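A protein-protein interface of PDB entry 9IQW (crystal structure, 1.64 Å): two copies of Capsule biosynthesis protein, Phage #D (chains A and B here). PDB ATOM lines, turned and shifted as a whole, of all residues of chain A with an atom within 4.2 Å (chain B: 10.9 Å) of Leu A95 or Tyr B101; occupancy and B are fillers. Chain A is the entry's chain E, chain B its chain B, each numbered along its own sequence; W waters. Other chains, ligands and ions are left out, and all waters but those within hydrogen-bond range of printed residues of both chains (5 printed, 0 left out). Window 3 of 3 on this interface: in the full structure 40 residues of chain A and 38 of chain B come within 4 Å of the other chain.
The side-chain amide nitrogen (ND2) of Asn A15 lies within hydrogen-bond range of the backbone carbonyl oxygen (O) of Val B100, at 3.1 Å. OD2 of Asp B102 is in hydrogen-bond range of N of Asn A15, at 2.8 Å. N of Cys A17 sits at hydrogen-bond distance from O of Trp B103 (3.0 Å). The backbone carbonyl oxygen (O) of Lys A108 sits at hydrogen-bond distance from the backbone NH (N) of Ile B104 (2.9 Å). O of Cys A17 sits at hydrogen-bond distance from N of Ile B105 (2.7 Å).
O of Leu A16 is in hydrogen-bond range of N of Thr A57 (2.9 Å). The backbone carbonyl oxygen (O) of Leu A58 lies within hydrogen-bond range of the backbone NH (N) of Leu A95 (2.8 Å). The backbone carbonyl oxygen of Leu A95 is in hydrogen-bond range of the backbone NH of Thr A60.
Among the printed residues, merely in contact across the chains: Cys A17 with Ile B104 (3.3 Å), Lys A108 with Trp B103 (3.4 Å), Lys A108 with Asp B102 (3.4 Å), Asn A15 with Tyr B101 (3.5 Å), Cys A17 with Tyr B101 (3.6 Å), Leu A95 with Tyr B101 (3.6 Å), Leu A16 with Trp B103 (3.7 Å), Thr A57 with Tyr B101 (3.7 Å), Asn A15 with Trp B103 (3.7 Å) and Lys A108 with Tyr B101 (3.9 Å).
Leu A95 touches just one residue of chain B: Tyr B101. Of chain A, only Asn A15, Cys A17, Thr A57, Leu A95 and Lys A108 come within 4 Å of Tyr B101. Of chain B, only Val B100, Tyr B101, Asp B102 and Trp B103 come within 4 Å of Asn A15. Of chain B, only Tyr B101 (3.7 Å) comes within 4 Å of Thr A57. No residue of chain B comes within 4 Å of Thr A60. No residue of chain B comes within 4 Å of Thr A96. Printed residues of chain A within 4 Å of Asp B102: Asn A15 and Lys A108. Of the printed residues of chain B, Leu A16 touches Trp B103 (3.7 Å). The nearest residue of chain B that does not touch Leu A95 is Pro B99 (6.6 Å).
Printed residues of chain B that touch a printed residue of chain A: Val B100, Tyr B101, Asp B102, Trp B103, Ile B104 and Ile B105. Of the 11 printed residues of chain A, 6 touch a printed residue of chain B. Among the printed residues, 15 pairs touch across the chains.
2 positions are printed for both chains.
Water W2 bridges the side-chain carboxylate (OD1) of Asp B102 (2.7 Å) and the side-chain amino group (NZ) of Lys A108 (2.8 Å). Water W3 bridges the side-chain hydroxyl of Thr A57 and the side-chain hydroxyl of Tyr B101. Water W5 lies within hydrogen-bond range of OH of Tyr B59 (2.9 Å) and OH of Tyr A59 (3.0 Å). Water W4 bridges the backbone carbonyl oxygen (O) of Val B100 (2.9 Å) and the side-chain amide nitrogen (ND2) of Asn A15 (3.3 Å). Water W1 bridges O of Ile B105 and O of Cys A17.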
ATOM      1  N   ASN A  15      -2.762   5.210   4.902  1.00  0.00           N
ATOM      2  CA  ASN A  15      -2.916   4.143   5.880  1.00  0.00           C
ATOM      3  C   ASN A  15      -2.830   2.831   5.108  1.00  0.00           C
ATOM      4  O   ASN A  15      -3.779   2.474   4.412  1.00  0.00           O
ATOM      5  CB  ASN A  15      -4.268   4.296   6.572  1.00  0.00           C
ATOM      6  CG  ASN A  15      -4.535   3.318   7.655  1.00  0.00           C
ATOM      7  OD1 ASN A  15      -3.609   2.792   8.291  1.00  0.00           O
ATOM      8  ND2 ASN A  15      -5.833   3.099   7.912  1.00  0.00           N
ATOM      9  N   LEU A  16      -1.679   2.156   5.193  1.00  0.00           N
ATOM     10  CA  LEU A  16      -1.365   1.042   4.302  1.00  0.00           C
ATOM     11  C   LEU A  16      -1.296  -0.281   5.055  1.00  0.00           C
ATOM     12  O   LEU A  16      -0.771  -0.330   6.171  1.00  0.00           O
ATOM     13  CB  LEU A  16      -0.013   1.298   3.622  1.00  0.00           C
ATOM     14  CG  LEU A  16       0.138   2.595   2.896  1.00  0.00           C
ATOM     15  CD1 LEU A  16       1.538   2.793   2.401  1.00  0.00           C
ATOM     16  CD2 LEU A  16      -0.829   2.696   1.737  1.00  0.00           C
ATOM     17  N   CYS A  17      -1.778  -1.351   4.414  1.00  0.00           N
ATOM     18  CA  CYS A  17      -1.784  -2.689   4.979  1.00  0.00           C
ATOM     19  C   CYS A  17      -1.094  -3.681   4.044  1.00  0.00           C
ATOM     20  O   CYS A  17      -1.503  -3.820   2.895  1.00  0.00           O
ATOM     21  CB  CYS A  17      -3.219  -3.107   5.250  1.00  0.00           C
ATOM     22  SG  CYS A  17      -3.387  -4.705   6.075  1.00  0.00           S
ATOM     23  N   THR A  57       0.988  -0.999   8.359  1.00  0.00           N
ATOM     24  CA  THR A  57       0.424  -2.132   9.071  1.00  0.00           C
ATOM     25  C   THR A  57       0.770  -3.406   8.317  1.00  0.00           C
ATOM     26  O   THR A  57       0.609  -3.468   7.099  1.00  0.00           O
ATOM     27  CB  THR A  57      -1.088  -2.017   9.230  1.00  0.00           C
ATOM     28  OG1 THR A  57      -1.386  -0.865  10.035  1.00  0.00           O
ATOM     29  CG2 THR A  57      -1.706  -3.267   9.857  1.00  0.00           C
ATOM     30  N   LEU A  58       1.262  -4.394   9.064  1.00  0.00           N
ATOM     31  CA  LEU A  58       1.462  -5.737   8.555  1.00  0.00           C
ATOM     32  C   LEU A  58       0.333  -6.620   9.075  1.00  0.00           C
ATOM     33  O   LEU A  58      -0.060  -6.518  10.239  1.00  0.00           O
ATOM     34  CB  LEU A  58       2.802  -6.285   9.024  1.00  0.00           C
ATOM     35  CG  LEU A  58       4.021  -5.381   8.828  1.00  0.00           C
ATOM     36  CD1 LEU A  58       5.274  -6.143   9.163  1.00  0.00           C
ATOM     37  CD2 LEU A  58       4.091  -4.819   7.437  1.00  0.00           C
ATOM     38  N   TYR A  59      -0.181  -7.488   8.198  1.00  0.00           N
ATOM     39  CA  TYR A  59      -1.341  -8.307   8.503  1.00  0.00           C
ATOM     40  C   TYR A  59      -1.078  -9.704   7.961  1.00  0.00           C
ATOM     41  O   TYR A  59      -0.778  -9.863   6.776  1.00  0.00           O
ATOM     42  CB  TYR A  59      -2.561  -7.670   7.848  1.00  0.00           C
ATOM     43  CG  TYR A  59      -3.935  -8.186   8.215  1.00  0.00           C
ATOM     44  CD1 TYR A  59      -4.176  -8.802   9.438  1.00  0.00           C
ATOM     45  CD2 TYR A  59      -4.997  -8.062   7.330  1.00  0.00           C
ATOM     46  CE1 TYR A  59      -5.450  -9.249   9.783  1.00  0.00           C
ATOM     47  CE2 TYR A  59      -6.268  -8.508   7.659  1.00  0.00           C
ATOM     48  CZ  TYR A  59      -6.495  -9.100   8.885  1.00  0.00           C
ATOM     49  OH  TYR A  59      -7.761  -9.555   9.181  1.00  0.00           O
ATOM     50  N   THR A  60      -1.144 -10.711   8.838  1.00  0.00           N
ATOM     51  CA  THR A  60      -0.761 -12.055   8.441  1.00  0.00           C
ATOM     52  C   THR A  60      -1.757 -13.124   8.875  1.00  0.00           C
ATOM     53  O   THR A  60      -2.347 -13.048   9.956  1.00  0.00           O
ATOM     54  CB  THR A  60       0.651 -12.389   8.945  1.00  0.00           C
ATOM     55  OG1 THR A  60       1.084 -13.632   8.377  1.00  0.00           O
ATOM     56  CG2 THR A  60       0.717 -12.494  10.445  1.00  0.00           C
ATOM     57  N   LEU A  94       1.350  -4.573  13.762  1.00  0.00           N
ATOM     58  CA  LEU A  94       1.373  -5.968  13.360  1.00  0.00           C
ATOM     59  C   LEU A  94       0.108  -6.650  13.857  1.00  0.00           C
ATOM     60  O   LEU A  94      -0.148  -6.689  15.066  1.00  0.00           O
ATOM     61  CB  LEU A  94       2.621  -6.664  13.907  1.00  0.00           C
ATOM     62  CG  LEU A  94       2.728  -8.162  13.636  1.00  0.00           C
ATOM     63  CD1 LEU A  94       2.723  -8.465  12.168  1.00  0.00           C
ATOM     64  CD2 LEU A  94       3.977  -8.733  14.234  1.00  0.00           C
ATOM     65  N   LEU A  95      -0.686  -7.153  12.899  1.00  0.00           N
ATOM     66  CA  LEU A  95      -1.934  -7.826  13.191  1.00  0.00           C
ATOM     67  C   LEU A  95      -1.913  -9.255  12.649  1.00  0.00           C
ATOM     68  O   LEU A  95      -1.353  -9.511  11.584  1.00  0.00           O
ATOM     69  CB  LEU A  95      -3.105  -7.053  12.568  1.00  0.00           C
ATOM     70  CG  LEU A  95      -3.239  -5.598  12.956  1.00  0.00           C
ATOM     71  CD1 LEU A  95      -4.326  -4.915  12.148  1.00  0.00           C
ATOM     72  CD2 LEU A  95      -3.515  -5.472  14.423  1.00  0.00           C
ATOM     73  N   THR A  96      -2.542 -10.159  13.410  1.00  0.00           N
ATOM     74  CA  THR A  96      -2.615 -11.575  13.089  1.00  0.00           C
ATOM     75  C   THR A  96      -4.058 -12.005  12.832  1.00  0.00           C
ATOM     76  O   THR A  96      -4.960 -11.173  12.790  1.00  0.00           O
ATOM     77  CB  THR A  96      -1.951 -12.368  14.216  1.00  0.00           C
ATOM     78  OG1 THR A  96      -2.674 -12.186  15.441  1.00  0.00           O
ATOM     79  CG2 THR A  96      -0.476 -11.973  14.413  1.00  0.00           C
ATOM     80  N   LYS A 108      -9.564  -1.086  -3.444  1.00  0.00           N
ATOM     81  CA  LYS A 108      -8.326  -0.498  -2.956  1.00  0.00           C
ATOM     82  C   LYS A 108      -7.304  -1.577  -2.608  1.00  0.00           C
ATOM     83  O   LYS A 108      -6.695  -1.559  -1.535  1.00  0.00           O
ATOM     84  CB  LYS A 108      -8.609   0.398  -1.740  1.00  0.00           C
ATOM     85  CG  LYS A 108      -9.365   1.639  -2.102  1.00  0.00           C
ATOM     86  CD  LYS A 108      -9.760   2.499  -0.914  1.00  0.00           C
ATOM     87  CE  LYS A 108     -10.530   3.715  -1.364  1.00  0.00           C
ATOM     88  NZ  LYS A 108     -10.871   4.575  -0.220  1.00  0.00           N
ATOM     89  N   ASP B  19     -15.615  -6.957  -1.951  1.00  0.00           N
ATOM     90  CA  ASP B  19     -16.183  -5.725  -1.435  1.00  0.00           C
ATOM     91  C   ASP B  19     -17.574  -5.522  -2.027  1.00  0.00           C
ATOM     92  O   ASP B  19     -17.861  -5.974  -3.134  1.00  0.00           O
ATOM     93  CB  ASP B  19     -15.326  -4.505  -1.786  1.00  0.00           C
ATOM     94  CG  ASP B  19     -14.146  -4.242  -0.890  1.00  0.00           C
ATOM     95  OD1 ASP B  19     -13.676  -5.200  -0.236  1.00  0.00           O
ATOM     96  OD2 ASP B  19     -13.725  -3.053  -0.797  1.00  0.00           O
ATOM     97  N   ASP B  21     -19.202  -2.009  -1.683  1.00  0.00           N
ATOM     98  CA  ASP B  21     -19.206  -0.640  -2.161  1.00  0.00           C
ATOM     99  C   ASP B  21     -18.082  -0.350  -3.158  1.00  0.00           C
ATOM    100  O   ASP B  21     -16.960  -0.808  -2.990  1.00  0.00           O
ATOM    101  CB  ASP B  21     -19.151   0.313  -0.966  1.00  0.00           C
ATOM    102  CG  ASP B  21     -20.459   0.304  -0.195  1.00  0.00           C
ATOM    103  OD1 ASP B  21     -21.524   0.394  -0.840  1.00  0.00           O
ATOM    104  OD2 ASP B  21     -20.413   0.200   1.063  1.00  0.00           O
ATOM    105  N   TYR B  59     -17.898  -8.718   1.907  1.00  0.00           N
ATOM    106  CA  TYR B  59     -17.254  -8.147   3.077  1.00  0.00           C
ATOM    107  C   TYR B  59     -17.310  -6.630   2.958  1.00  0.00           C
ATOM    108  O   TYR B  59     -16.875  -6.071   1.952  1.00  0.00           O
ATOM    109  CB  TYR B  59     -15.816  -8.655   3.117  1.00  0.00           C
ATOM    110  CG  TYR B  59     -14.997  -8.427   4.362  1.00  0.00           C
ATOM    111  CD1 TYR B  59     -15.596  -8.275   5.607  1.00  0.00           C
ATOM    112  CD2 TYR B  59     -13.612  -8.379   4.299  1.00  0.00           C
ATOM    113  CE1 TYR B  59     -14.828  -8.105   6.764  1.00  0.00           C
ATOM    114  CE2 TYR B  59     -12.838  -8.208   5.442  1.00  0.00           C
ATOM    115  CZ  TYR B  59     -13.446  -8.076   6.673  1.00  0.00           C
ATOM    116  OH  TYR B  59     -12.644  -7.889   7.773  1.00  0.00           O
ATOM    117  N   THR B  60     -17.873  -5.956   3.964  1.00  0.00           N
ATOM    118  CA  THR B  60     -18.063  -4.522   3.872  1.00  0.00           C
ATOM    119  C   THR B  60     -17.645  -3.762   5.127  1.00  0.00           C
ATOM    120  O   THR B  60     -17.823  -4.240   6.259  1.00  0.00           O
ATOM    121  CB  THR B  60     -19.533  -4.195   3.503  1.00  0.00           C
ATOM    122  OG1 THR B  60     -19.656  -2.807   3.234  1.00  0.00           O
ATOM    123  CG2 THR B  60     -20.498  -4.569   4.604  1.00  0.00           C
ATOM    124  N   ALA B  61     -17.129  -2.551   4.884  1.00  0.00           N
ATOM    125  CA  ALA B  61     -16.831  -1.582   5.934  1.00  0.00           C
ATOM    126  C   ALA B  61     -17.983  -0.615   6.187  1.00  0.00           C
ATOM    127  O   ALA B  61     -17.887   0.296   7.019  1.00  0.00           O
ATOM    128  CB  ALA B  61     -15.583  -0.799   5.548  1.00  0.00           C
ATOM    129  N   ARG B  62     -19.088  -0.809   5.468  1.00  0.00           N
ATOM    130  CA  ARG B  62     -20.149   0.183   5.477  1.00  0.00           C
ATOM    131  C   ARG B  62     -20.664   0.375   6.893  1.00  0.00           C
ATOM    132  O   ARG B  62     -20.972  -0.598   7.576  1.00  0.00           O
ATOM    133  CB  ARG B  62     -21.308  -0.208   4.553  1.00  0.00           C
ATOM    134  CG  ARG B  62     -22.269   0.933   4.330  1.00  0.00           C
ATOM    135  CD  ARG B  62     -23.488   0.479   3.578  1.00  0.00           C
ATOM    136  NE  ARG B  62     -23.191   0.063   2.215  1.00  0.00           N
ATOM    137  CZ  ARG B  62     -24.081  -0.503   1.406  1.00  0.00           C
ATOM    138  NH1 ARG B  62     -25.333  -0.700   1.798  1.00  0.00           N
ATOM    139  NH2 ARG B  62     -23.712  -0.852   0.171  1.00  0.00           N
ATOM    140  N   MET B  64     -19.109   1.687   9.529  1.00  0.00           N
ATOM    141  CA  MET B  64     -18.147   1.665  10.617  1.00  0.00           C
ATOM    142  C   MET B  64     -17.873   3.080  11.116  1.00  0.00           C
ATOM    143  O   MET B  64     -17.726   3.292  12.316  1.00  0.00           O
ATOM    144  CB  MET B  64     -16.849   0.969  10.186  1.00  0.00           C
ATOM    145  CG  MET B  64     -17.023  -0.528  10.059  1.00  0.00           C
ATOM    146  SD  MET B  64     -17.190  -1.311  11.684  1.00  0.00           S
ATOM    147  CE  MET B  64     -15.483  -1.469  12.061  1.00  0.00           C
ATOM    148  N   LYS B  65     -17.839   4.048  10.189  1.00  0.00           N
ATOM    149  CA  LYS B  65     -17.616   5.444  10.546  1.00  0.00           C
ATOM    150  C   LYS B  65     -18.898   6.246  10.762  1.00  0.00           C
ATOM    151  O   LYS B  65     -18.922   7.159  11.581  1.00  0.00           O
ATOM    152  CB  LYS B  65     -16.750   6.115   9.475  1.00  0.00           C
ATOM    153  CG  LYS B  65     -15.352   5.483   9.380  1.00  0.00           C
ATOM    154  CD  LYS B  65     -14.487   6.050   8.266  1.00  0.00           C
ATOM    155  CE  LYS B  65     -13.139   5.365   8.200  1.00  0.00           C
ATOM    156  NZ  LYS B  65     -12.242   6.007   7.201  1.00  0.00           N
ATOM    157  N   HIS B  97     -17.943  -5.092   9.478  1.00  0.00           N
ATOM    158  CA  HIS B  97     -16.867  -4.621  10.325  1.00  0.00           C
ATOM    159  C   HIS B  97     -15.497  -4.738   9.665  1.00  0.00           C
ATOM    160  O   HIS B  97     -14.487  -4.914  10.339  1.00  0.00           O
ATOM    161  CB  HIS B  97     -16.909  -5.315  11.709  1.00  0.00           C
ATOM    162  CG  HIS B  97     -18.163  -5.025  12.478  1.00  0.00           C
ATOM    163  ND1 HIS B  97     -19.379  -5.575  12.116  1.00  0.00           N
ATOM    164  CD2 HIS B  97     -18.347  -4.258  13.586  1.00  0.00           C
ATOM    165  CE1 HIS B  97     -20.271  -5.115  12.998  1.00  0.00           C
ATOM    166  NE2 HIS B  97     -19.692  -4.310  13.901  1.00  0.00           N
ATOM    167  N   LYS B  98     -15.465  -4.594   8.335  1.00  0.00           N
ATOM    168  CA  LYS B  98     -14.207  -4.601   7.609  1.00  0.00           C
ATOM    169  C   LYS B  98     -13.389  -3.374   8.010  1.00  0.00           C
ATOM    170  O   LYS B  98     -13.908  -2.258   8.065  1.00  0.00           O
ATOM    171  CB  LYS B  98     -14.464  -4.578   6.109  1.00  0.00           C
ATOM    172  CG  LYS B  98     -13.184  -4.644   5.273  1.00  0.00           C
ATOM    173  CD  LYS B  98     -13.436  -4.414   3.790  1.00  0.00           C
ATOM    174  CE  LYS B  98     -12.103  -4.395   3.064  1.00  0.00           C
ATOM    175  NZ  LYS B  98     -12.219  -3.894   1.687  1.00  0.00           N
ATOM    176  N   PRO B  99     -12.073  -3.533   8.291  1.00  0.00           N
ATOM    177  CA  PRO B  99     -11.232  -2.375   8.558  1.00  0.00           C
ATOM    178  C   PRO B  99     -10.998  -1.563   7.289  1.00  0.00           C
ATOM    179  O   PRO B  99     -11.185  -2.067   6.188  1.00  0.00           O
ATOM    180  CB  PRO B  99      -9.942  -2.985   9.127  1.00  0.00           C
ATOM    181  CG  PRO B  99      -9.910  -4.384   8.585  1.00  0.00           C
ATOM    182  CD  PRO B  99     -11.353  -4.816   8.346  1.00  0.00           C
ATOM    183  N   VAL B 100     -10.648  -0.290   7.466  1.00  0.00           N
ATOM    184  CA  VAL B 100     -10.450   0.607   6.343  1.00  0.00           C
ATOM    185  C   VAL B 100      -8.972   0.966   6.203  1.00  0.00           C
ATOM    186  O   VAL B 100      -8.357   1.463   7.149  1.00  0.00           O
ATOM    187  CB  VAL B 100     -11.325   1.868   6.507  1.00  0.00           C
ATOM    188  CG1 VAL B 100     -11.027   2.892   5.421  1.00  0.00           C
ATOM    189  CG2 VAL B 100     -12.816   1.494   6.531  1.00  0.00           C
ATOM    190  N   TYR B 101      -8.438   0.719   4.997  1.00  0.00           N
ATOM    191  CA  TYR B 101      -7.111   1.166   4.612  1.00  0.00           C
ATOM    192  C   TYR B 101      -7.203   1.887   3.273  1.00  0.00           C
ATOM    193  O   TYR B 101      -8.120   1.630   2.489  1.00  0.00           O
ATOM    194  CB  TYR B 101      -6.168  -0.037   4.483  1.00  0.00           C
ATOM    195  CG  TYR B 101      -5.939  -0.770   5.791  1.00  0.00           C
ATOM    196  CD1 TYR B 101      -5.043  -0.289   6.731  1.00  0.00           C
ATOM    197  CD2 TYR B 101      -6.606  -1.949   6.071  1.00  0.00           C
ATOM    198  CE1 TYR B 101      -4.842  -0.948   7.942  1.00  0.00           C
ATOM    199  CE2 TYR B 101      -6.416  -2.618   7.276  1.00  0.00           C
ATOM    200  CZ  TYR B 101      -5.525  -2.122   8.204  1.00  0.00           C
ATOM    201  OH  TYR B 101      -5.321  -2.788   9.384  1.00  0.00           O
ATOM    202  N   ASP B 102      -6.239   2.766   3.005  1.00  0.00           N
ATOM    203  CA  ASP B 102      -6.132   3.377   1.683  1.00  0.00           C
ATOM    204  C   ASP B 102      -5.734   2.349   0.626  1.00  0.00           C
ATOM    205  O   ASP B 102      -6.191   2.423  -0.516  1.00  0.00           O
ATOM    206  CB  ASP B 102      -5.175   4.538   1.697  1.00  0.00           C
ATOM    207  CG  ASP B 102      -5.687   5.686   2.554  1.00  0.00           C
ATOM    208  OD1 ASP B 102      -6.827   6.174   2.279  1.00  0.00           O
ATOM    209  OD2 ASP B 102      -4.970   6.091   3.504  1.00  0.00           O
ATOM    210  N   TRP B 103      -4.864   1.412   1.017  1.00  0.00           N
ATOM    211  CA  TRP B 103      -4.470   0.300   0.171  1.00  0.00           C
ATOM    212  C   TRP B 103      -4.194  -0.941   1.002  1.00  0.00           C
ATOM    213  O   TRP B 103      -3.582  -0.837   2.064  1.00  0.00           O
ATOM    214  CB  TRP B 103      -3.188   0.614  -0.622  1.00  0.00           C
ATOM    215  CG  TRP B 103      -3.369   1.633  -1.698  1.00  0.00           C
ATOM    216  CD1 TRP B 103      -2.997   2.937  -1.668  1.00  0.00           C
ATOM    217  CD2 TRP B 103      -4.010   1.428  -2.953  1.00  0.00           C
ATOM    218  NE1 TRP B 103      -3.352   3.557  -2.837  1.00  0.00           N
ATOM    219  CE2 TRP B 103      -3.964   2.648  -3.651  1.00  0.00           C
ATOM    220  CE3 TRP B 103      -4.588   0.319  -3.575  1.00  0.00           C
ATOM    221  CZ2 TRP B 103      -4.499   2.795  -4.938  1.00  0.00           C
ATOM    222  CZ3 TRP B 103      -5.105   0.468  -4.856  1.00  0.00           C
ATOM    223  CH2 TRP B 103      -5.042   1.687  -5.520  1.00  0.00           C
ATOM    224  N   ILE B 104      -4.612  -2.094   0.467  1.00  0.00           N
ATOM    225  CA  ILE B 104      -4.123  -3.387   0.906  1.00  0.00           C
ATOM    226  C   ILE B 104      -3.184  -3.899  -0.180  1.00  0.00           C
ATOM    227  O   ILE B 104      -3.564  -3.932  -1.348  1.00  0.00           O
ATOM    228  CB  ILE B 104      -5.286  -4.372   1.141  1.00  0.00           C
ATOM    229  CG1 ILE B 104      -5.986  -4.092   2.494  1.00  0.00           C
ATOM    230  CG2 ILE B 104      -4.846  -5.807   1.061  1.00  0.00           C
ATOM    231  CD1 ILE B 104      -7.427  -4.695   2.578  1.00  0.00           C
ATOM    232  N   ILE B 105      -1.966  -4.261   0.223  1.00  0.00           N
ATOM    233  CA  ILE B 105      -0.991  -4.866  -0.660  1.00  0.00           C
ATOM    234  C   ILE B 105      -0.939  -6.335  -0.268  1.00  0.00           C
ATOM    235  O   ILE B 105      -0.553  -6.675   0.842  1.00  0.00           O
ATOM    236  CB  ILE B 105       0.373  -4.173  -0.591  1.00  0.00           C
ATOM    237  CG1 ILE B 105       0.272  -2.682  -0.944  1.00  0.00           C
ATOM    238  CG2 ILE B 105       1.367  -4.880  -1.512  1.00  0.00           C
ATOM    239  CD1 ILE B 105      -0.156  -1.784   0.171  1.00  0.00           C
ATOM    240  N   ASP B 106      -1.344  -7.199  -1.205  1.00  0.00           N
ATOM    241  CA  ASP B 106      -1.712  -8.564  -0.880  1.00  0.00           C
ATOM    242  C   ASP B 106      -1.423  -9.409  -2.120  1.00  0.00           C
ATOM    243  O   ASP B 106      -1.774  -8.996  -3.217  1.00  0.00           O
ATOM    244  CB  ASP B 106      -3.206  -8.564  -0.484  1.00  0.00           C
ATOM    245  CG  ASP B 106      -3.855  -9.875  -0.122  1.00  0.00           C
ATOM    246  OD1 ASP B 106      -3.470 -10.907  -0.698  1.00  0.00           O
ATOM    247  OD2 ASP B 106      -4.761  -9.877   0.779  1.00  0.00           O
ATOM    248  N   ARG B 111      -8.410  -5.913  -8.249  1.00  0.00           N
ATOM    249  CA  ARG B 111      -9.428  -4.876  -8.292  1.00  0.00           C
ATOM    250  C   ARG B 111     -10.535  -5.294  -9.253  1.00  0.00           C
ATOM    251  O   ARG B 111     -10.353  -6.208 -10.065  1.00  0.00           O
ATOM    252  CB  ARG B 111      -8.820  -3.513  -8.650  1.00  0.00           C
ATOM    253  CG  ARG B 111      -7.811  -3.023  -7.616  1.00  0.00           C
ATOM    254  CD  ARG B 111      -7.428  -1.572  -7.790  1.00  0.00           C
ATOM    255  NE  ARG B 111      -6.684  -1.313  -9.022  1.00  0.00           N
ATOM    256  CZ  ARG B 111      -5.386  -1.517  -9.188  1.00  0.00           C
ATOM    257  NH1 ARG B 111      -4.630  -1.996  -8.215  1.00  0.00           N
ATOM    258  NH2 ARG B 111      -4.823  -1.207 -10.357  1.00  0.00           N
HETATM  259  O   HOH W   1      -2.603  -6.973   3.192  1.00  0.00           O
HETATM  260  O   HOH W   2      -8.434   5.933   0.185  1.00  0.00           O
HETATM  261  O   HOH W   3      -3.762  -0.751  11.440  1.00  0.00           O
HETATM  262  O   HOH W   4      -7.422   1.018   9.875  1.00  0.00           O
HETATM  263  O   HOH W   5      -9.930  -8.602   7.267  1.00  0.00           O
